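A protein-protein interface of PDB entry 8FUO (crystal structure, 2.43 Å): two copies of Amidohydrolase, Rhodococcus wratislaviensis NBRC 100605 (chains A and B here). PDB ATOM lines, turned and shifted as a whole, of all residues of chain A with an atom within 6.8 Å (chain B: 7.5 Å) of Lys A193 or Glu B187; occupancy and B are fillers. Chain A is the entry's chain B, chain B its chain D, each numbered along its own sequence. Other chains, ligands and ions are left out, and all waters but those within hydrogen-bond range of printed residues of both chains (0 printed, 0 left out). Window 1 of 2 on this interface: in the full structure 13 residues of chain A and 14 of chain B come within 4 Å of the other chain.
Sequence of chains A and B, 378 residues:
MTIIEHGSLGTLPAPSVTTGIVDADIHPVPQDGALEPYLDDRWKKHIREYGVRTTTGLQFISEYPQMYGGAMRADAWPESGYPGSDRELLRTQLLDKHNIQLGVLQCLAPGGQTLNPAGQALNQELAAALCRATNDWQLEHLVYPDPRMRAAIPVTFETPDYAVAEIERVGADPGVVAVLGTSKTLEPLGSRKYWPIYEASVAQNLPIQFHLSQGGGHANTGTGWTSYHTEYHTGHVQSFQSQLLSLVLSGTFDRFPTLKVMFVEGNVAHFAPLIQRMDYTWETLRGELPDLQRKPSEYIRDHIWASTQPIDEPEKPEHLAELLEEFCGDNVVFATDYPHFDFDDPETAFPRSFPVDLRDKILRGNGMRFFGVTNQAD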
ATOM      1  N   THR A 156      15.997 -28.170 -10.016  1.00  0.00           N
ATOM      2  CA  THR A 156      16.730 -26.969 -10.422  1.00  0.00           C
ATOM      3  C   THR A 156      15.720 -25.900 -10.826  1.00  0.00           C
ATOM      4  O   THR A 156      15.328 -25.794 -11.988  1.00  0.00           O
ATOM      5  CB  THR A 156      17.698 -27.264 -11.569  1.00  0.00           C
ATOM      6  OG1 THR A 156      17.012 -27.924 -12.641  1.00  0.00           O
ATOM      7  CG2 THR A 156      18.883 -28.134 -11.113  1.00  0.00           C
ATOM      8  N   PHE A 157      15.292 -25.077  -9.858  1.00  0.00           N
ATOM      9  CA  PHE A 157      14.352 -24.013 -10.212  1.00  0.00           C
ATOM     10  C   PHE A 157      14.940 -23.055 -11.244  1.00  0.00           C
ATOM     11  O   PHE A 157      14.193 -22.478 -12.043  1.00  0.00           O
ATOM     12  CB  PHE A 157      13.891 -23.247  -8.964  1.00  0.00           C
ATOM     13  CG  PHE A 157      12.727 -23.896  -8.258  1.00  0.00           C
ATOM     14  CD1 PHE A 157      12.918 -24.982  -7.426  1.00  0.00           C
ATOM     15  CD2 PHE A 157      11.442 -23.430  -8.452  1.00  0.00           C
ATOM     16  CE1 PHE A 157      11.856 -25.576  -6.814  1.00  0.00           C
ATOM     17  CE2 PHE A 157      10.367 -24.028  -7.831  1.00  0.00           C
ATOM     18  CZ  PHE A 157      10.575 -25.098  -7.013  1.00  0.00           C
ATOM     19  N   GLU A 158      16.264 -22.888 -11.264  1.00  0.00           N
ATOM     20  CA  GLU A 158      16.885 -21.949 -12.192  1.00  0.00           C
ATOM     21  C   GLU A 158      16.997 -22.493 -13.615  1.00  0.00           C
ATOM     22  O   GLU A 158      17.291 -21.715 -14.529  1.00  0.00           O
ATOM     23  CB  GLU A 158      18.260 -21.516 -11.668  1.00  0.00           C
ATOM     24  CG  GLU A 158      18.208 -20.753 -10.326  1.00  0.00           C
ATOM     25  CD  GLU A 158      17.326 -19.478 -10.356  1.00  0.00           C
ATOM     26  OE1 GLU A 158      16.601 -19.213 -11.345  1.00  0.00           O
ATOM     27  OE2 GLU A 158      17.369 -18.709  -9.371  1.00  0.00           O
ATOM     28  N   THR A 159      16.750 -23.792 -13.821  1.00  0.00           N
ATOM     29  CA  THR A 159      16.587 -24.382 -15.150  1.00  0.00           C
ATOM     30  C   THR A 159      15.262 -25.127 -15.161  1.00  0.00           C
ATOM     31  O   THR A 159      15.212 -26.338 -14.900  1.00  0.00           O
ATOM     32  CB  THR A 159      17.745 -25.310 -15.506  1.00  0.00           C
ATOM     33  OG1 THR A 159      18.966 -24.760 -14.990  1.00  0.00           O
ATOM     34  CG2 THR A 159      17.862 -25.454 -17.033  1.00  0.00           C
ATOM     35  N   PRO A 160      14.165 -24.424 -15.459  1.00  0.00           N
ATOM     36  CA  PRO A 160      12.834 -25.056 -15.429  1.00  0.00           C
ATOM     37  C   PRO A 160      12.666 -26.277 -16.335  1.00  0.00           C
ATOM     38  O   PRO A 160      11.731 -27.053 -16.115  1.00  0.00           O
ATOM     39  CB  PRO A 160      11.900 -23.915 -15.869  1.00  0.00           C
ATOM     40  CG  PRO A 160      12.603 -22.669 -15.456  1.00  0.00           C
ATOM     41  CD  PRO A 160      14.084 -22.952 -15.553  1.00  0.00           C
ATOM     42  N   LEU A 186      17.400 -16.050  -8.668  1.00  0.00           N
ATOM     43  CA  LEU A 186      17.899 -14.949  -9.515  1.00  0.00           C
ATOM     44  C   LEU A 186      16.789 -13.977  -9.915  1.00  0.00           C
ATOM     45  O   LEU A 186      17.016 -12.764 -10.011  1.00  0.00           O
ATOM     46  CB  LEU A 186      18.560 -15.498 -10.775  1.00  0.00           C
ATOM     47  CG  LEU A 186      19.279 -14.465 -11.664  1.00  0.00           C
ATOM     48  CD1 LEU A 186      20.634 -14.019 -11.037  1.00  0.00           C
ATOM     49  CD2 LEU A 186      19.501 -15.002 -13.087  1.00  0.00           C
ATOM     50  N   GLU A 187      15.607 -14.491 -10.183  1.00  0.00           N
ATOM     51  CA  GLU A 187      14.395 -13.710 -10.306  1.00  0.00           C
ATOM     52  C   GLU A 187      13.445 -14.037  -9.147  1.00  0.00           C
ATOM     53  O   GLU A 187      13.439 -15.163  -8.642  1.00  0.00           O
ATOM     54  CB  GLU A 187      13.695 -13.996 -11.639  1.00  0.00           C
ATOM     55  CG  GLU A 187      14.476 -13.538 -12.843  1.00  0.00           C
ATOM     56  CD  GLU A 187      14.066 -14.223 -14.139  1.00  0.00           C
ATOM     57  OE1 GLU A 187      12.901 -14.068 -14.587  1.00  0.00           O
ATOM     58  OE2 GLU A 187      14.931 -14.911 -14.726  1.00  0.00           O
ATOM     59  N   PRO A 188      12.641 -13.077  -8.697  1.00  0.00           N
ATOM     60  CA  PRO A 188      11.634 -13.387  -7.670  1.00  0.00           C
ATOM     61  C   PRO A 188      10.624 -14.424  -8.163  1.00  0.00           C
ATOM     62  O   PRO A 188      10.234 -14.437  -9.332  1.00  0.00           O
ATOM     63  CB  PRO A 188      10.971 -12.034  -7.407  1.00  0.00           C
ATOM     64  CG  PRO A 188      11.959 -11.003  -7.892  1.00  0.00           C
ATOM     65  CD  PRO A 188      12.667 -11.646  -9.053  1.00  0.00           C
ATOM     66  N   LEU A 189      10.174 -15.278  -7.242  1.00  0.00           N
ATOM     67  CA  LEU A 189       9.491 -16.521  -7.611  1.00  0.00           C
ATOM     68  C   LEU A 189       8.175 -16.309  -8.366  1.00  0.00           C
ATOM     69  O   LEU A 189       7.699 -17.244  -9.021  1.00  0.00           O
ATOM     70  CB  LEU A 189       9.275 -17.372  -6.363  1.00  0.00           C
ATOM     71  CG  LEU A 189      10.521 -18.135  -5.912  1.00  0.00           C
ATOM     72  CD1 LEU A 189      10.288 -18.743  -4.569  1.00  0.00           C
ATOM     73  CD2 LEU A 189      10.899 -19.202  -6.936  1.00  0.00           C
ATOM     74  N   GLY A 190       7.599 -15.111  -8.332  1.00  0.00           N
ATOM     75  CA  GLY A 190       6.445 -14.851  -9.168  1.00  0.00           C
ATOM     76  C   GLY A 190       6.759 -14.629 -10.639  1.00  0.00           C
ATOM     77  O   GLY A 190       5.842 -14.453 -11.458  1.00  0.00           O
ATOM     78  N   SER A 191       8.047 -14.646 -10.993  1.00  0.00           N
ATOM     79  CA  SER A 191       8.443 -14.467 -12.382  1.00  0.00           C
ATOM     80  C   SER A 191       7.911 -15.615 -13.231  1.00  0.00           C
ATOM     81  O   SER A 191       7.867 -16.764 -12.786  1.00  0.00           O
ATOM     82  CB  SER A 191       9.967 -14.373 -12.501  1.00  0.00           C
ATOM     83  OG  SER A 191      10.486 -13.318 -11.711  1.00  0.00           O
ATOM     84  N   ARG A 192       7.504 -15.286 -14.463  1.00  0.00           N
ATOM     85  CA  ARG A 192       7.037 -16.283 -15.425  1.00  0.00           C
ATOM     86  C   ARG A 192       8.074 -17.381 -15.680  1.00  0.00           C
ATOM     87  O   ARG A 192       7.707 -18.513 -15.993  1.00  0.00           O
ATOM     88  CB  ARG A 192       6.654 -15.576 -16.734  1.00  0.00           C
ATOM     89  CG  ARG A 192       5.776 -16.378 -17.611  1.00  0.00           C
ATOM     90  CD  ARG A 192       5.612 -15.689 -18.935  1.00  0.00           C
ATOM     91  NE  ARG A 192       4.758 -16.468 -19.815  1.00  0.00           N
ATOM     92  CZ  ARG A 192       3.428 -16.417 -19.789  1.00  0.00           C
ATOM     93  NH1 ARG A 192       2.720 -17.167 -20.626  1.00  0.00           N
ATOM     94  NH2 ARG A 192       2.805 -15.619 -18.927  1.00  0.00           N
ATOM     95  N   LYS A 193       9.366 -17.074 -15.542  1.00  0.00           N
ATOM     96  CA  LYS A 193      10.402 -18.098 -15.615  1.00  0.00           C
ATOM     97  C   LYS A 193      10.048 -19.397 -14.890  1.00  0.00           C
ATOM     98  O   LYS A 193      10.323 -20.487 -15.405  1.00  0.00           O
ATOM     99  CB  LYS A 193      11.716 -17.593 -15.042  1.00  0.00           C
ATOM    100  CG  LYS A 193      12.738 -18.719 -14.972  1.00  0.00           C
ATOM    101  CD  LYS A 193      14.129 -18.269 -14.606  1.00  0.00           C
ATOM    102  CE  LYS A 193      15.000 -19.486 -14.341  1.00  0.00           C
ATOM    103  NZ  LYS A 193      16.386 -19.117 -13.980  1.00  0.00           N
ATOM    104  N   TYR A 194       9.455 -19.297 -13.692  1.00  0.00           N
ATOM    105  CA  TYR A 194       9.222 -20.468 -12.845  1.00  0.00           C
ATOM    106  C   TYR A 194       7.837 -21.077 -13.018  1.00  0.00           C
ATOM    107  O   TYR A 194       7.583 -22.143 -12.463  1.00  0.00           O
ATOM    108  CB  TYR A 194       9.443 -20.123 -11.354  1.00  0.00           C
ATOM    109  CG  TYR A 194      10.788 -19.458 -11.063  1.00  0.00           C
ATOM    110  CD1 TYR A 194      11.974 -20.195 -11.022  1.00  0.00           C
ATOM    111  CD2 TYR A 194      10.866 -18.083 -10.858  1.00  0.00           C
ATOM    112  CE1 TYR A 194      13.189 -19.572 -10.769  1.00  0.00           C
ATOM    113  CE2 TYR A 194      12.076 -17.460 -10.610  1.00  0.00           C
ATOM    114  CZ  TYR A 194      13.227 -18.203 -10.565  1.00  0.00           C
ATOM    115  OH  TYR A 194      14.402 -17.552 -10.313  1.00  0.00           O
ATOM    116  N   TRP A 195       6.948 -20.429 -13.760  1.00  0.00           N
ATOM    117  CA  TRP A 195       5.633 -21.002 -14.011  1.00  0.00           C
ATOM    118  C   TRP A 195       5.685 -22.411 -14.586  1.00  0.00           C
ATOM    119  O   TRP A 195       4.843 -23.231 -14.191  1.00  0.00           O
ATOM    120  CB  TRP A 195       4.808 -20.080 -14.925  1.00  0.00           C
ATOM    121  CG  TRP A 195       4.363 -18.842 -14.236  1.00  0.00           C
ATOM    122  CD1 TRP A 195       4.872 -18.339 -13.080  1.00  0.00           C
ATOM    123  CD2 TRP A 195       3.311 -17.950 -14.631  1.00  0.00           C
ATOM    124  NE1 TRP A 195       4.219 -17.182 -12.735  1.00  0.00           N
ATOM    125  CE2 TRP A 195       3.261 -16.916 -13.671  1.00  0.00           C
ATOM    126  CE3 TRP A 195       2.411 -17.918 -15.704  1.00  0.00           C
ATOM    127  CZ2 TRP A 195       2.345 -15.860 -13.745  1.00  0.00           C
ATOM    128  CZ3 TRP A 195       1.513 -16.872 -15.782  1.00  0.00           C
ATOM    129  CH2 TRP A 195       1.482 -15.858 -14.810  1.00  0.00           C
ATOM    130  N   PRO A 196       6.601 -22.770 -15.486  1.00  0.00           N
ATOM    131  CA  PRO A 196       6.632 -24.170 -15.930  1.00  0.00           C
ATOM    132  C   PRO A 196       6.779 -25.147 -14.785  1.00  0.00           C
ATOM    133  O   PRO A 196       6.251 -26.261 -14.859  1.00  0.00           O
ATOM    134  CB  PRO A 196       7.835 -24.212 -16.882  1.00  0.00           C
ATOM    135  CG  PRO A 196       7.906 -22.825 -17.423  1.00  0.00           C
ATOM    136  CD  PRO A 196       7.510 -21.923 -16.289  1.00  0.00           C
ATOM    137  N   ILE A 197       7.461 -24.760 -13.716  1.00  0.00           N
ATOM    138  CA  ILE A 197       7.587 -25.649 -12.567  1.00  0.00           C
ATOM    139  C   ILE A 197       6.270 -25.738 -11.810  1.00  0.00           C
ATOM    140  O   ILE A 197       5.847 -26.823 -11.392  1.00  0.00           O
ATOM    141  CB  ILE A 197       8.742 -25.176 -11.674  1.00  0.00           C
ATOM    142  CG1 ILE A 197       9.934 -24.786 -12.561  1.00  0.00           C
ATOM    143  CG2 ILE A 197       9.148 -26.282 -10.731  1.00  0.00           C
ATOM    144  CD1 ILE A 197      11.284 -24.844 -11.857  1.00  0.00           C
ATOM    145  N   GLU B 158      14.074 -11.345 -21.760  1.00  0.00           N
ATOM    146  CA  GLU B 158      13.930 -11.841 -20.400  1.00  0.00           C
ATOM    147  C   GLU B 158      12.550 -12.417 -20.109  1.00  0.00           C
ATOM    148  O   GLU B 158      12.313 -12.841 -18.976  1.00  0.00           O
ATOM    149  CB  GLU B 158      14.275 -10.747 -19.376  1.00  0.00           C
ATOM    150  CG  GLU B 158      15.731 -10.192 -19.452  1.00  0.00           C
ATOM    151  CD  GLU B 158      16.821 -11.215 -19.126  1.00  0.00           C
ATOM    152  OE1 GLU B 158      16.564 -12.432 -19.060  1.00  0.00           O
ATOM    153  OE2 GLU B 158      17.966 -10.783 -18.918  1.00  0.00           O
ATOM    154  N   THR B 159      11.634 -12.426 -21.090  1.00  0.00           N
ATOM    155  CA  THR B 159      10.465 -13.312 -21.094  1.00  0.00           C
ATOM    156  C   THR B 159      10.424 -13.996 -22.455  1.00  0.00           C
ATOM    157  O   THR B 159       9.803 -13.491 -23.402  1.00  0.00           O
ATOM    158  CB  THR B 159       9.165 -12.567 -20.816  1.00  0.00           C
ATOM    159  OG1 THR B 159       9.327 -11.758 -19.656  1.00  0.00           O
ATOM    160  CG2 THR B 159       8.053 -13.562 -20.560  1.00  0.00           C
ATOM    161  N   PRO B 160      11.125 -15.123 -22.602  1.00  0.00           N
ATOM    162  CA  PRO B 160      11.218 -15.774 -23.926  1.00  0.00           C
ATOM    163  C   PRO B 160       9.874 -16.121 -24.552  1.00  0.00           C
ATOM    164  O   PRO B 160       9.711 -16.026 -25.780  1.00  0.00           O
ATOM    165  CB  PRO B 160      12.038 -17.028 -23.620  1.00  0.00           C
ATOM    166  CG  PRO B 160      12.913 -16.611 -22.457  1.00  0.00           C
ATOM    167  CD  PRO B 160      12.168 -15.579 -21.663  1.00  0.00           C
ATOM    168  N   SER B 183      23.009  -5.909 -25.028  1.00  0.00           N
ATOM    169  CA  SER B 183      24.287  -6.480 -24.599  1.00  0.00           C
ATOM    170  C   SER B 183      24.269  -6.955 -23.145  1.00  0.00           C
ATOM    171  O   SER B 183      25.040  -7.856 -22.774  1.00  0.00           O
ATOM    172  CB  SER B 183      25.415  -5.453 -24.784  1.00  0.00           C
ATOM    173  OG  SER B 183      25.151  -4.223 -24.101  1.00  0.00           O
ATOM    174  N   LYS B 184      23.453  -6.339 -22.292  1.00  0.00           N
ATOM    175  CA  LYS B 184      23.397  -6.716 -20.885  1.00  0.00           C
ATOM    176  C   LYS B 184      22.116  -7.498 -20.617  1.00  0.00           C
ATOM    177  O   LYS B 184      21.051  -7.178 -21.170  1.00  0.00           O
ATOM    178  CB  LYS B 184      23.499  -5.482 -19.977  1.00  0.00           C
ATOM    179  CG  LYS B 184      24.853  -4.812 -20.083  1.00  0.00           C
ATOM    180  CD  LYS B 184      25.039  -3.677 -19.115  1.00  0.00           C
ATOM    181  CE  LYS B 184      26.485  -3.129 -19.193  1.00  0.00           C
ATOM    182  NZ  LYS B 184      26.834  -2.725 -20.571  1.00  0.00           N
ATOM    183  N   THR B 185      22.245  -8.555 -19.807  1.00  0.00           N
ATOM    184  CA  THR B 185      21.151  -9.469 -19.503  1.00  0.00           C
ATOM    185  C   THR B 185      21.343 -10.012 -18.102  1.00  0.00           C
ATOM    186  O   THR B 185      22.427  -9.919 -17.520  1.00  0.00           O
ATOM    187  CB  THR B 185      21.072 -10.641 -20.488  1.00  0.00           C
ATOM    188  OG1 THR B 185      22.307 -11.377 -20.461  1.00  0.00           O
ATOM    189  CG2 THR B 185      20.782 -10.165 -21.883  1.00  0.00           C
ATOM    190  N   LEU B 186      20.272 -10.613 -17.565  1.00  0.00           N
ATOM    191  CA  LEU B 186      20.327 -11.118 -16.194  1.00  0.00           C
ATOM    192  C   LEU B 186      21.160 -12.394 -16.090  1.00  0.00           C
ATOM    193  O   LEU B 186      21.869 -12.596 -15.099  1.00  0.00           O
ATOM    194  CB  LEU B 186      18.906 -11.358 -15.667  1.00  0.00           C
ATOM    195  CG  LEU B 186      18.833 -11.583 -14.158  1.00  0.00           C
ATOM    196  CD1 LEU B 186      19.333 -10.357 -13.422  1.00  0.00           C
ATOM    197  CD2 LEU B 186      17.401 -11.899 -13.752  1.00  0.00           C
ATOM    198  N   GLU B 187      21.064 -13.278 -17.076  1.00  0.00           N
ATOM    199  CA  GLU B 187      21.990 -14.396 -17.198  1.00  0.00           C
ATOM    200  C   GLU B 187      22.847 -14.223 -18.457  1.00  0.00           C
ATOM    201  O   GLU B 187      22.464 -13.507 -19.392  1.00  0.00           O
ATOM    202  CB  GLU B 187      21.250 -15.748 -17.249  1.00  0.00           C
ATOM    203  CG  GLU B 187      19.914 -15.776 -16.474  1.00  0.00           C
ATOM    204  CD  GLU B 187      19.204 -17.140 -16.436  1.00  0.00           C
ATOM    205  OE1 GLU B 187      19.874 -18.185 -16.509  1.00  0.00           O
ATOM    206  OE2 GLU B 187      17.962 -17.155 -16.299  1.00  0.00           O
ATOM    207  N   PRO B 188      24.036 -14.828 -18.494  1.00  0.00           N
ATOM    208  CA  PRO B 188      24.816 -14.839 -19.734  1.00  0.00           C
ATOM    209  C   PRO B 188      24.021 -15.483 -20.867  1.00  0.00           C
ATOM    210  O   PRO B 188      23.390 -16.529 -20.686  1.00  0.00           O
ATOM    211  CB  PRO B 188      26.040 -15.669 -19.358  1.00  0.00           C
ATOM    212  CG  PRO B 188      26.187 -15.457 -17.900  1.00  0.00           C
ATOM    213  CD  PRO B 188      24.788 -15.427 -17.379  1.00  0.00           C
ATOM    214  N   LEU B 189      24.057 -14.843 -22.043  1.00  0.00           N
ATOM    215  CA  LEU B 189      23.218 -15.249 -23.171  1.00  0.00           C
ATOM    216  C   LEU B 189      23.418 -16.702 -23.598  1.00  0.00           C
ATOM    217  O   LEU B 189      22.560 -17.245 -24.306  1.00  0.00           O
ATOM    218  CB  LEU B 189      23.472 -14.323 -24.352  1.00  0.00           C
ATOM    219  CG  LEU B 189      22.836 -12.930 -24.282  1.00  0.00           C
ATOM    220  CD1 LEU B 189      23.404 -11.993 -25.368  1.00  0.00           C
ATOM    221  CD2 LEU B 189      21.313 -13.029 -24.397  1.00  0.00           C
ATOM    222  N   GLY B 190      24.516 -17.352 -23.193  1.00  0.00           N
ATOM    223  CA  GLY B 190      24.666 -18.780 -23.440  1.00  0.00           C
ATOM    224  C   GLY B 190      23.791 -19.682 -22.593  1.00  0.00           C
ATOM    225  O   GLY B 190      23.816 -20.900 -22.775  1.00  0.00           O
ATOM    226  N   SER B 191      23.000 -19.113 -21.695  1.00  0.00           N
ATOM    227  CA  SER B 191      22.161 -19.878 -20.790  1.00  0.00           C
ATOM    228  C   SER B 191      20.911 -20.386 -21.499  1.00  0.00           C
ATOM    229  O   SER B 191      20.363 -19.731 -22.396  1.00  0.00           O
ATOM    230  CB  SER B 191      21.784 -19.017 -19.580  1.00  0.00           C
ATOM    231  OG  SER B 191      20.631 -19.505 -18.921  1.00  0.00           O
ATOM    232  N   ARG B 192      20.464 -21.573 -21.067  1.00  0.00           N
ATOM    233  CA  ARG B 192      19.309 -22.214 -21.680  1.00  0.00           C
ATOM    234  C   ARG B 192      18.060 -21.344 -21.662  1.00  0.00           C
ATOM    235  O   ARG B 192      17.158 -21.576 -22.479  1.00  0.00           O
ATOM    236  CB  ARG B 192      19.024 -23.541 -20.980  1.00  0.00           C
ATOM    237  CG  ARG B 192      20.062 -24.609 -21.276  1.00  0.00           C
ATOM    238  CD  ARG B 192      19.712 -25.904 -20.582  1.00  0.00           C
ATOM    239  NE  ARG B 192      18.484 -26.522 -21.073  1.00  0.00           N
ATOM    240  CZ  ARG B 192      18.430 -27.396 -22.080  1.00  0.00           C
ATOM    241  NH1 ARG B 192      19.537 -27.758 -22.716  1.00  0.00           N
ATOM    242  NH2 ARG B 192      17.264 -27.905 -22.455  1.00  0.00           N
ATOM    243  N   LYS B 193      17.983 -20.353 -20.764  1.00  0.00           N
ATOM    244  CA  LYS B 193      16.802 -19.494 -20.696  1.00  0.00           C
ATOM    245  C   LYS B 193      16.413 -18.942 -22.072  1.00  0.00           C
ATOM    246  O   LYS B 193      15.223 -18.859 -22.406  1.00  0.00           O
ATOM    247  CB  LYS B 193      17.034 -18.341 -19.708  1.00  0.00           C
ATOM    248  CG  LYS B 193      15.823 -17.410 -19.620  1.00  0.00           C
ATOM    249  CD  LYS B 193      15.967 -16.192 -18.718  1.00  0.00           C
ATOM    250  CE  LYS B 193      14.748 -15.286 -18.959  1.00  0.00           C
ATOM    251  NZ  LYS B 193      14.685 -14.091 -18.099  1.00  0.00           N
ATOM    252  N   TYR B 194      17.411 -18.590 -22.889  1.00  0.00           N
ATOM    253  CA  TYR B 194      17.200 -17.876 -24.145  1.00  0.00           C
ATOM    254  C   TYR B 194      17.140 -18.778 -25.379  1.00  0.00           C
ATOM    255  O   TYR B 194      16.760 -18.290 -26.449  1.00  0.00           O
ATOM    256  CB  TYR B 194      18.309 -16.828 -24.338  1.00  0.00           C
ATOM    257  CG  TYR B 194      18.491 -15.924 -23.136  1.00  0.00           C
ATOM    258  CD1 TYR B 194      17.523 -14.965 -22.800  1.00  0.00           C
ATOM    259  CD2 TYR B 194      19.622 -16.027 -22.331  1.00  0.00           C
ATOM    260  CE1 TYR B 194      17.688 -14.137 -21.695  1.00  0.00           C
ATOM    261  CE2 TYR B 194      19.796 -15.201 -21.215  1.00  0.00           C
ATOM    262  CZ  TYR B 194      18.822 -14.256 -20.897  1.00  0.00           C
ATOM    263  OH  TYR B 194      18.987 -13.430 -19.788  1.00  0.00           O
ATOM    264  N   GLY B 216      19.972  -4.327 -17.401  1.00  0.00           N
ATOM    265  CA  GLY B 216      20.216  -5.751 -17.474  1.00  0.00           C
ATOM    266  C   GLY B 216      20.029  -6.475 -16.164  1.00  0.00           C
ATOM    267  O   GLY B 216      19.559  -7.619 -16.150  1.00  0.00           O
ATOM    268  N   HIS B 218      22.706  -6.302 -13.473  1.00  0.00           N
ATOM    269  CA  HIS B 218      23.933  -6.225 -12.689  1.00  0.00           C
ATOM    270  C   HIS B 218      24.616  -4.879 -12.884  1.00  0.00           C
ATOM    271  O   HIS B 218      24.196  -4.051 -13.703  1.00  0.00           O
ATOM    272  CB  HIS B 218      24.875  -7.367 -13.067  1.00  0.00           C
ATOM    273  CG  HIS B 218      24.197  -8.695 -13.078  1.00  0.00           C
ATOM    274  ND1 HIS B 218      24.093  -9.487 -11.951  1.00  0.00           N
ATOM    275  CD2 HIS B 218      23.556  -9.357 -14.072  1.00  0.00           C
ATOM    276  CE1 HIS B 218      23.433 -10.590 -12.262  1.00  0.00           C
ATOM    277  NE2 HIS B 218      23.088 -10.530 -13.540  1.00  0.00           N
ATOM    278  N   GLN B 243      29.666 -12.010 -22.969  1.00  0.00           N
ATOM    279  CA  GLN B 243      28.599 -12.721 -23.678  1.00  0.00           C
ATOM    280  C   GLN B 243      29.129 -13.695 -24.727  1.00  0.00           C
ATOM    281  O   GLN B 243      28.494 -14.722 -24.993  1.00  0.00           O
ATOM    282  CB  GLN B 243      27.644 -11.719 -24.343  1.00  0.00           C
ATOM    283  CG  GLN B 243      26.896 -10.746 -23.387  1.00  0.00           C
ATOM    284  CD  GLN B 243      25.652 -11.339 -22.730  1.00  0.00           C
ATOM    285  OE1 GLN B 243      25.599 -12.520 -22.400  1.00  0.00           O
ATOM    286  NE2 GLN B 243      24.645 -10.505 -22.532  1.00  0.00           N
ATOM    287  N   SER B 246      30.275 -16.977 -22.956  1.00  0.00           N
ATOM    288  CA  SER B 246      29.153 -17.821 -22.566  1.00  0.00           C
ATOM    289  C   SER B 246      28.463 -18.426 -23.788  1.00  0.00           C
ATOM    290  O   SER B 246      28.170 -19.622 -23.806  1.00  0.00           O
ATOM    291  CB  SER B 246      28.176 -17.024 -21.712  1.00  0.00           C
ATOM    292  OG  SER B 246      26.877 -17.585 -21.751  1.00  0.00           O
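Of the 17 printed residues of chain A, 4 touch a printed residue of chain B. Hydrophobic or aromatic side chains of chain A within 4 Å of the printed part of chain B: Leu A186. Along chain A the printed residues that touch a printed residue of chain B span positions 186 to 193. Printed residues of chain B that touch a printed residue of chain A: Thr B159, Leu B186, Glu B187 and Lys B193. Hydrophobic or aromatic side chains of chain B that line the printed part of chain A: Leu B186. Among the printed residues, 6 pairs touch across the chains. Among the printed residues, Asp or Glu carboxylates within 4 Å of a Lys or Arg side-chain nitrogen of the other chain: Glu A187 with Lys B193 (3.5 Å) and Lys A193 with Glu B187 (3.4 Å).
Lys A193 touches just one residue of chain B: Glu B187. Glu B187 touches two residues of chain A. Of the printed residues of chain A, Lys B193 touches Glu A187 (3.5 Å). Of the printed residues of chain A, Leu B186 touches Leu A186 (3.6 Å) and Glu A187 (3.5 Å). Of the printed residues of chain B, Leu A186 touches Leu B186 and Glu B187. Of the printed residues of chain A, Thr B159 touches Arg A192. Printed residues of chain B within 4 Å of Arg A192: Thr B159 (3.6 Å). Ser A191 touches none of the printed residues of chain B. The nearest residue of chain B that does not touch Lys A193 is Lys B193 (5.0 Å). The nearest residue of chain A that does not touch Glu B187 is Glu A187 (4.1 Å).
CG of Leu B186 touches CD2 of Leu A186, at 3.6 Å. Glu B187 touches Leu A186 (CG to CD2, 3.5 Å). Glu A187 touches Leu B186 (CG to CD2, 3.5 Å). CG2 of Thr B159 touches CD of Arg A192 (3.6 Å).
The side-chain carboxylate (OE2) of Glu A158 lies within hydrogen-bond range of the backbone NH (N) of Leu A186 (2.8 Å). The side-chain carboxylate (OE2) of Glu B158 is in hydrogen-bond range of the backbone NH (N) of Leu B186. The side-chain carboxylate (OE1) of Glu B158 lies within salt-bridge range of the side-chain amino group (NZ) of Lys B193 (2.7 Å). The backbone NH (N) of Leu B186 lies within hydrogen-bond range of the backbone carbonyl oxygen (O) of Gly B216 (3.4 Å). The backbone carbonyl oxygen (O) of Leu B186 lies within hydrogen-bond range of a ring nitrogen (NE2) of His B218, at 2.9 Å. The backbone NH of Lys B193 lies close to the side-chain hydroxyl of Ser B191 (3.3 Å).
The side-chain carboxylate (OE2) of Glu A187 is in salt-bridge range of the side-chain amino group (NZ) of Lys B193 (3.5 Å). The side-chain carboxylate of Glu B187 is in salt-bridge range of the side-chain amino group of Lys A193 (3.4 Å).
Leu B186 touches its own counterpart, Leu A186. Leu A186 touches Glu B187, and with the chains exchanged Glu A187 touches Leu B186. Glu A187 touches Lys B193, and with the chains exchanged Lys A193 touches Glu B187. Arg A192 touches Thr B159, but with the chains exchanged Thr A159 does not touch Arg B192 (4.03 Å). 12 positions are printed for both chains. Of the 6 pairs that touch across the chains among the printed residues, 5 have their exchanged pair printed and touching as well.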
